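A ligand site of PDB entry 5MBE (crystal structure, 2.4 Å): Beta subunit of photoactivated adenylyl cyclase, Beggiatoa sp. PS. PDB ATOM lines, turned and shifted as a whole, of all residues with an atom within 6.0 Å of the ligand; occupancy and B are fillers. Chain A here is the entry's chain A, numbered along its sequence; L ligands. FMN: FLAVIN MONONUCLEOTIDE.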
ATOM      1  N   TYR A  10      20.372 -37.831  33.385  1.00  0.00           N
ATOM      2  CA  TYR A  10      21.254 -38.221  32.289  1.00  0.00           C
ATOM      3  C   TYR A  10      22.486 -37.333  32.280  1.00  0.00           C
ATOM      4  O   TYR A  10      22.454 -36.184  32.740  1.00  0.00           O
ATOM      5  CB  TYR A  10      20.547 -38.156  30.923  1.00  0.00           C
ATOM      6  CG  TYR A  10      20.394 -36.757  30.347  1.00  0.00           C
ATOM      7  CD1 TYR A  10      21.366 -36.222  29.510  1.00  0.00           C
ATOM      8  CD2 TYR A  10      19.262 -35.995  30.618  1.00  0.00           C
ATOM      9  CE1 TYR A  10      21.223 -34.951  28.970  1.00  0.00           C
ATOM     10  CE2 TYR A  10      19.120 -34.724  30.079  1.00  0.00           C
ATOM     11  CZ  TYR A  10      20.104 -34.211  29.261  1.00  0.00           C
ATOM     12  OH  TYR A  10      19.967 -32.953  28.724  1.00  0.00           O
ATOM     13  N   SER A  12      25.748 -36.146  29.505  1.00  0.00           N
ATOM     14  CA  SER A  12      26.049 -36.061  28.088  1.00  0.00           C
ATOM     15  C   SER A  12      27.373 -35.344  27.883  1.00  0.00           C
ATOM     16  O   SER A  12      27.973 -34.809  28.824  1.00  0.00           O
ATOM     17  CB  SER A  12      24.931 -35.346  27.323  1.00  0.00           C
ATOM     18  OG  SER A  12      24.927 -33.955  27.592  1.00  0.00           O
ATOM     19  N   ILE A  26      20.272 -21.987  26.055  1.00  0.00           N
ATOM     20  CA  ILE A  26      19.624 -23.271  26.292  1.00  0.00           C
ATOM     21  C   ILE A  26      18.753 -23.199  27.543  1.00  0.00           C
ATOM     22  O   ILE A  26      17.613 -23.691  27.550  1.00  0.00           O
ATOM     23  CB  ILE A  26      20.691 -24.383  26.415  1.00  0.00           C
ATOM     24  CG1 ILE A  26      21.580 -24.406  25.169  1.00  0.00           C
ATOM     25  CG2 ILE A  26      20.024 -25.739  26.610  1.00  0.00           C
ATOM     26  CD1 ILE A  26      22.704 -25.414  25.235  1.00  0.00           C
ATOM     27  N   VAL A  29      15.563 -20.955  26.866  1.00  0.00           N
ATOM     28  CA  VAL A  29      14.507 -21.705  26.181  1.00  0.00           C
ATOM     29  C   VAL A  29      13.956 -22.793  27.091  1.00  0.00           C
ATOM     30  O   VAL A  29      12.762 -23.095  27.065  1.00  0.00           O
ATOM     31  CB  VAL A  29      15.044 -22.282  24.863  1.00  0.00           C
ATOM     32  CG1 VAL A  29      13.941 -23.012  24.113  1.00  0.00           C
ATOM     33  CG2 VAL A  29      15.646 -21.178  23.999  1.00  0.00           C
ATOM     34  N   SER A  30      14.811 -23.388  27.932  1.00  0.00           N
ATOM     35  CA  SER A  30      14.363 -24.437  28.828  1.00  0.00           C
ATOM     36  C   SER A  30      13.351 -23.899  29.842  1.00  0.00           C
ATOM     37  O   SER A  30      12.352 -24.561  30.146  1.00  0.00           O
ATOM     38  CB  SER A  30      15.556 -25.062  29.545  1.00  0.00           C
ATOM     39  OG  SER A  30      16.528 -25.508  28.622  1.00  0.00           O
ATOM     40  N   ILE A  31      13.591 -22.694  30.365  1.00  0.00           N
ATOM     41  CA  ILE A  31      12.672 -22.113  31.335  1.00  0.00           C
ATOM     42  C   ILE A  31      11.307 -21.868  30.702  1.00  0.00           C
ATOM     43  O   ILE A  31      10.267 -22.087  31.336  1.00  0.00           O
ATOM     44  CB  ILE A  31      13.274 -20.819  31.934  1.00  0.00           C
ATOM     45  CG1 ILE A  31      14.555 -21.124  32.697  1.00  0.00           C
ATOM     46  CG2 ILE A  31      12.273 -20.136  32.850  1.00  0.00           C
ATOM     47  CD1 ILE A  31      15.375 -19.900  33.047  1.00  0.00           C
ATOM     48  N   ASN A  33       9.868 -23.445  28.072  1.00  0.00           N
ATOM     49  CA  ASN A  33       9.136 -24.653  27.702  1.00  0.00           C
ATOM     50  C   ASN A  33       8.835 -25.528  28.916  1.00  0.00           C
ATOM     51  O   ASN A  33       7.753 -26.127  28.998  1.00  0.00           O
ATOM     52  CB  ASN A  33       9.925 -25.452  26.662  1.00  0.00           C
ATOM     53  CG  ASN A  33      10.037 -24.720  25.337  1.00  0.00           C
ATOM     54  OD1 ASN A  33      11.010 -24.010  25.082  1.00  0.00           O
ATOM     55  ND2 ASN A  33       9.040 -24.899  24.476  1.00  0.00           N
ATOM     56  N   ASN A  34       9.766 -25.620  29.870  1.00  0.00           N
ATOM     57  CA  ASN A  34       9.539 -26.470  31.026  1.00  0.00           C
ATOM     58  C   ASN A  34       8.477 -25.888  31.953  1.00  0.00           C
ATOM     59  O   ASN A  34       7.766 -26.643  32.626  1.00  0.00           O
ATOM     60  CB  ASN A  34      10.844 -26.687  31.789  1.00  0.00           C
ATOM     61  CG  ASN A  34      11.844 -27.512  31.005  1.00  0.00           C
ATOM     62  OD1 ASN A  34      11.632 -27.809  29.829  1.00  0.00           O
ATOM     63  ND2 ASN A  34      12.955 -27.868  31.648  1.00  0.00           N
ATOM     64  N   ASP A  37       5.206 -26.609  30.300  1.00  0.00           N
ATOM     65  CA  ASP A  37       4.989 -28.043  30.404  1.00  0.00           C
ATOM     66  C   ASP A  37       4.829 -28.511  31.845  1.00  0.00           C
ATOM     67  O   ASP A  37       4.666 -29.723  32.067  1.00  0.00           O
ATOM     68  CB  ASP A  37       6.147 -28.804  29.754  1.00  0.00           C
ATOM     69  CG  ASP A  37       6.143 -28.711  28.236  1.00  0.00           C
ATOM     70  OD1 ASP A  37       5.040 -28.778  27.645  1.00  0.00           O
ATOM     71  OD2 ASP A  37       7.229 -28.566  27.639  1.00  0.00           O
ATOM     72  N   LEU A  43      19.911 -28.302  35.436  1.00  0.00           N
ATOM     73  CA  LEU A  43      20.911 -28.535  34.406  1.00  0.00           C
ATOM     74  C   LEU A  43      22.268 -28.030  34.882  1.00  0.00           C
ATOM     75  O   LEU A  43      22.384 -26.859  35.272  1.00  0.00           O
ATOM     76  CB  LEU A  43      20.528 -27.857  33.084  1.00  0.00           C
ATOM     77  CG  LEU A  43      21.584 -27.875  31.973  1.00  0.00           C
ATOM     78  CD1 LEU A  43      21.896 -29.289  31.523  1.00  0.00           C
ATOM     79  CD2 LEU A  43      21.145 -27.013  30.800  1.00  0.00           C
ATOM     80  N   PHE A  50      27.387 -32.276  30.368  1.00  0.00           N
ATOM     81  CA  PHE A  50      26.104 -31.776  30.826  1.00  0.00           C
ATOM     82  C   PHE A  50      25.496 -32.746  31.838  1.00  0.00           C
ATOM     83  O   PHE A  50      25.496 -33.963  31.614  1.00  0.00           O
ATOM     84  CB  PHE A  50      25.142 -31.585  29.646  1.00  0.00           C
ATOM     85  CG  PHE A  50      25.267 -30.252  28.967  1.00  0.00           C
ATOM     86  CD1 PHE A  50      25.249 -29.080  29.702  1.00  0.00           C
ATOM     87  CD2 PHE A  50      25.407 -30.175  27.595  1.00  0.00           C
ATOM     88  CE1 PHE A  50      25.371 -27.852  29.078  1.00  0.00           C
ATOM     89  CE2 PHE A  50      25.528 -28.951  26.957  1.00  0.00           C
ATOM     90  CZ  PHE A  50      25.504 -27.787  27.703  1.00  0.00           C
ATOM     91  N   GLN A  52      21.887 -33.098  33.701  1.00  0.00           N
ATOM     92  CA  GLN A  52      20.529 -32.583  33.749  1.00  0.00           C
ATOM     93  C   GLN A  52      19.615 -33.589  34.442  1.00  0.00           C
ATOM     94  O   GLN A  52      19.665 -34.787  34.144  1.00  0.00           O
ATOM     95  CB  GLN A  52      19.997 -32.256  32.357  1.00  0.00           C
ATOM     96  CG  GLN A  52      18.636 -31.569  32.375  1.00  0.00           C
ATOM     97  CD  GLN A  52      18.257 -30.990  31.023  1.00  0.00           C
ATOM     98  OE1 GLN A  52      18.285 -31.690  30.009  1.00  0.00           O
ATOM     99  NE2 GLN A  52      17.895 -29.712  31.005  1.00  0.00           N
ATOM    100  N   LEU A  54      15.500 -34.192  35.106  1.00  0.00           N
ATOM    101  CA  LEU A  54      14.165 -33.808  34.680  1.00  0.00           C
ATOM    102  C   LEU A  54      13.137 -34.476  35.583  1.00  0.00           C
ATOM    103  O   LEU A  54      13.392 -35.524  36.177  1.00  0.00           O
ATOM    104  CB  LEU A  54      13.907 -34.198  33.218  1.00  0.00           C
ATOM    105  CG  LEU A  54      14.812 -33.544  32.169  1.00  0.00           C
ATOM    106  CD1 LEU A  54      14.338 -33.900  30.763  1.00  0.00           C
ATOM    107  CD2 LEU A  54      14.864 -32.042  32.349  1.00  0.00           C
ATOM    108  N   LEU A  64       9.731 -34.445  25.730  1.00  0.00           N
ATOM    109  CA  LEU A  64      10.809 -33.485  25.929  1.00  0.00           C
ATOM    110  C   LEU A  64      12.171 -34.165  25.840  1.00  0.00           C
ATOM    111  O   LEU A  64      13.098 -33.656  25.205  1.00  0.00           O
ATOM    112  CB  LEU A  64      10.648 -32.773  27.268  1.00  0.00           C
ATOM    113  CG  LEU A  64      11.869 -32.020  27.804  1.00  0.00           C
ATOM    114  CD1 LEU A  64      12.243 -30.866  26.890  1.00  0.00           C
ATOM    115  CD2 LEU A  64      11.612 -31.531  29.228  1.00  0.00           C
ATOM    116  N   LYS A  67      13.462 -34.969  22.298  1.00  0.00           N
ATOM    117  CA  LYS A  67      13.970 -33.847  21.513  1.00  0.00           C
ATOM    118  C   LYS A  67      15.367 -33.428  21.947  1.00  0.00           C
ATOM    119  O   LYS A  67      16.121 -32.876  21.134  1.00  0.00           O
ATOM    120  CB  LYS A  67      13.011 -32.657  21.602  1.00  0.00           C
ATOM    121  CG  LYS A  67      13.205 -31.647  20.485  1.00  0.00           C
ATOM    122  CD  LYS A  67      12.046 -30.660  20.424  1.00  0.00           C
ATOM    123  CE  LYS A  67      11.928 -30.046  19.030  1.00  0.00           C
ATOM    124  NZ  LYS A  67      13.220 -29.472  18.568  1.00  0.00           N
ATOM    125  N   ILE A  68      15.726 -33.678  23.204  1.00  0.00           N
ATOM    126  CA  ILE A  68      17.087 -33.396  23.656  1.00  0.00           C
ATOM    127  C   ILE A  68      18.079 -34.402  23.086  1.00  0.00           C
ATOM    128  O   ILE A  68      19.262 -34.101  22.957  1.00  0.00           O
ATOM    129  CB  ILE A  68      17.149 -33.359  25.191  1.00  0.00           C
ATOM    130  CG1 ILE A  68      15.982 -32.545  25.752  1.00  0.00           C
ATOM    131  CG2 ILE A  68      18.447 -32.746  25.667  1.00  0.00           C
ATOM    132  CD1 ILE A  68      15.947 -32.499  27.264  1.00  0.00           C
ATOM    133  N   ASP A  71      19.359 -33.300  19.688  1.00  0.00           N
ATOM    134  CA  ASP A  71      20.008 -31.993  19.721  1.00  0.00           C
ATOM    135  C   ASP A  71      21.427 -32.097  19.180  1.00  0.00           C
ATOM    136  O   ASP A  71      22.191 -32.983  19.563  1.00  0.00           O
ATOM    137  CB  ASP A  71      20.031 -31.457  21.150  1.00  0.00           C
ATOM    138  CG  ASP A  71      20.205 -29.955  21.213  1.00  0.00           C
ATOM    139  OD1 ASP A  71      21.346 -29.478  21.075  1.00  0.00           O
ATOM    140  OD2 ASP A  71      19.186 -29.247  21.390  1.00  0.00           O
ATOM    141  N   ARG A  73      23.933 -30.190  19.678  1.00  0.00           N
ATOM    142  CA  ARG A  73      24.962 -29.547  20.490  1.00  0.00           C
ATOM    143  C   ARG A  73      25.573 -30.468  21.539  1.00  0.00           C
ATOM    144  O   ARG A  73      26.614 -30.120  22.101  1.00  0.00           O
ATOM    145  CB  ARG A  73      24.369 -28.304  21.174  1.00  0.00           C
ATOM    146  CG  ARG A  73      24.018 -27.198  20.189  1.00  0.00           C
ATOM    147  CD  ARG A  73      23.012 -26.223  20.786  1.00  0.00           C
ATOM    148  NE  ARG A  73      21.741 -26.866  21.079  1.00  0.00           N
ATOM    149  CZ  ARG A  73      20.644 -26.225  21.478  1.00  0.00           C
ATOM    150  NH1 ARG A  73      20.673 -24.905  21.620  1.00  0.00           N
ATOM    151  NH2 ARG A  73      19.528 -26.889  21.712  1.00  0.00           N
ATOM    152  N   HIS A  74      24.965 -31.607  21.823  1.00  0.00           N
ATOM    153  CA  HIS A  74      25.547 -32.576  22.749  1.00  0.00           C
ATOM    154  C   HIS A  74      25.413 -33.969  22.175  1.00  0.00           C
ATOM    155  O   HIS A  74      24.491 -34.261  21.404  1.00  0.00           O
ATOM    156  CB  HIS A  74      24.908 -32.493  24.144  1.00  0.00           C
ATOM    157  CG  HIS A  74      23.471 -32.918  24.190  1.00  0.00           C
ATOM    158  ND1 HIS A  74      22.877 -33.425  25.321  1.00  0.00           N
ATOM    159  CD2 HIS A  74      22.511 -32.901  23.234  1.00  0.00           C
ATOM    160  CE1 HIS A  74      21.614 -33.707  25.069  1.00  0.00           C
ATOM    161  NE2 HIS A  74      21.369 -33.402  23.814  1.00  0.00           N
ATOM    162  N   ALA A  95      11.939 -24.396  37.204  1.00  0.00           N
ATOM    163  CA  ALA A  95      11.601 -24.838  35.861  1.00  0.00           C
ATOM    164  C   ALA A  95      12.814 -25.425  35.156  1.00  0.00           C
ATOM    165  O   ALA A  95      12.739 -26.491  34.533  1.00  0.00           O
ATOM    166  CB  ALA A  95      11.025 -23.668  35.052  1.00  0.00           C
ATOM    167  N   MET A  96      13.949 -24.739  35.256  1.00  0.00           N
ATOM    168  CA  MET A  96      15.238 -25.259  34.832  1.00  0.00           C
ATOM    169  C   MET A  96      16.358 -24.350  35.316  1.00  0.00           C
ATOM    170  O   MET A  96      16.639 -23.310  34.714  1.00  0.00           O
ATOM    171  CB  MET A  96      15.311 -25.396  33.304  1.00  0.00           C
ATOM    172  CG  MET A  96      16.621 -25.993  32.818  1.00  0.00           C
ATOM    173  SD  MET A  96      17.075 -27.479  33.735  1.00  0.00           S
ATOM    174  CE  MET A  96      15.710 -28.564  33.332  1.00  0.00           C
HETATM  175  N1  FMN L   1      14.677 -27.665  25.946  1.00  0.00           N
HETATM  176  C2  FMN L   1      13.595 -27.614  26.805  1.00  0.00           C
HETATM  177  O2  FMN L   1      12.536 -27.159  26.400  1.00  0.00           O
HETATM  178  N3  FMN L   1      13.710 -28.082  28.095  1.00  0.00           N
HETATM  179  C4  FMN L   1      14.909 -28.596  28.538  1.00  0.00           C
HETATM  180  O4  FMN L   1      15.014 -29.011  29.701  1.00  0.00           O
HETATM  181  C4A FMN L   1      16.002 -28.639  27.690  1.00  0.00           C
HETATM  182  N5  FMN L   1      17.192 -29.156  28.136  1.00  0.00           N
HETATM  183  C5A FMN L   1      18.272 -29.198  27.282  1.00  0.00           C
HETATM  184  C6  FMN L   1      19.470 -29.724  27.744  1.00  0.00           C
HETATM  185  C7  FMN L   1      20.568 -29.780  26.899  1.00  0.00           C
HETATM  186  C7M FMN L   1      21.867 -30.340  27.407  1.00  0.00           C
HETATM  187  C8  FMN L   1      20.470 -29.310  25.591  1.00  0.00           C
HETATM  188  C8M FMN L   1      21.661 -29.376  24.673  1.00  0.00           C
HETATM  189  C9  FMN L   1      19.265 -28.796  25.126  1.00  0.00           C
HETATM  190  C9A FMN L   1      18.166 -28.740  25.971  1.00  0.00           C
HETATM  191  N10 FMN L   1      16.967 -28.226  25.528  1.00  0.00           N
HETATM  192  C10 FMN L   1      15.881 -28.171  26.379  1.00  0.00           C
HETATM  193  C1' FMN L   1      16.848 -27.718  24.115  1.00  0.00           C
HETATM  194  C2' FMN L   1      15.966 -28.610  23.248  1.00  0.00           C
HETATM  195  O2' FMN L   1      16.745 -29.625  22.650  1.00  0.00           O
HETATM  196  C3' FMN L   1      15.262 -27.800  22.158  1.00  0.00           C
HETATM  197  O3' FMN L   1      16.032 -26.647  21.880  1.00  0.00           O
HETATM  198  C4' FMN L   1      13.868 -27.383  22.586  1.00  0.00           C
HETATM  199  O4' FMN L   1      13.278 -28.399  23.369  1.00  0.00           O
HETATM  200  C5' FMN L   1      12.980 -27.114  21.377  1.00  0.00           C
HETATM  201  O5' FMN L   1      13.182 -25.802  20.909  1.00  0.00           O
HETATM  202  P   FMN L   1      12.506 -25.305  19.527  1.00  0.00           P
HETATM  203  O1P FMN L   1      11.064 -25.751  19.528  1.00  0.00           O
HETATM  204  O2P FMN L   1      12.573 -23.803  19.444  1.00  0.00           O
HETATM  205  O3P FMN L   1      13.239 -25.924  18.353  1.00  0.00           O
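A nitrogen (N3) of the ligand sits at hydrogen-bond distance from the side-chain amide oxygen (OD1) of Asn 34 (2.7 Å). The side-chain carboxylate of Asp 71 sits at hydrogen-bond distance from an oxygen (O2') of the ligand (2.8 Å). The side-chain amide nitrogen (NE2) of Gln 52 is in hydrogen-bond range of a nitrogen (N5) of the ligand (3.0 Å). An oxygen (O3P) of the ligand is in salt-bridge range of the side-chain amino group (NZ) of Lys 67.
The side-chain amide oxygen (OD1) of Asn 34 lies close to the backbone carbonyl oxygen (O) of Ser 30, 3.3 Å away. O of Ala 95 lies within hydrogen-bond range of ND2 of Asn 34, at 3.2 Å. The guanidinium group (NH2) of Arg 73 is in salt-bridge range of the side-chain carboxylate (OD2) of Asp 71. The side-chain hydroxyl (OH) of Tyr 10 lies within hydrogen-bond range of the side-chain amide oxygen (OE1) of Gln 52, 2.5 Å away. The side-chain amide nitrogen (NE2) of Gln 52 sits close to the side-chain sulfur (SD) of Met 96 (3.6 Å). The backbone carbonyl oxygen (O) of Val 29 lies close to the side-chain amide oxygen (OD1) of Asn 33, at 2.8 Å. N of Phe 50 lies within hydrogen-bond range of O of Ser 12 (3.0 Å). N of Leu 43 sits at hydrogen-bond distance from SD of Met 96 (3.4 Å).
Merely in contact with the ligand: Asn 33, Ser 30, Leu 64, Tyr 10, Ile 26, Arg 73, Phe 50, Ile 68, Met 96 and His 74. Hydrophobic or aromatic side chains that line the ligand: Ile 26, Phe 50, Leu 64, Ile 68, His 74 and Met 96. Of the 21 residues printed, 14 come within 4 Å of the ligand.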
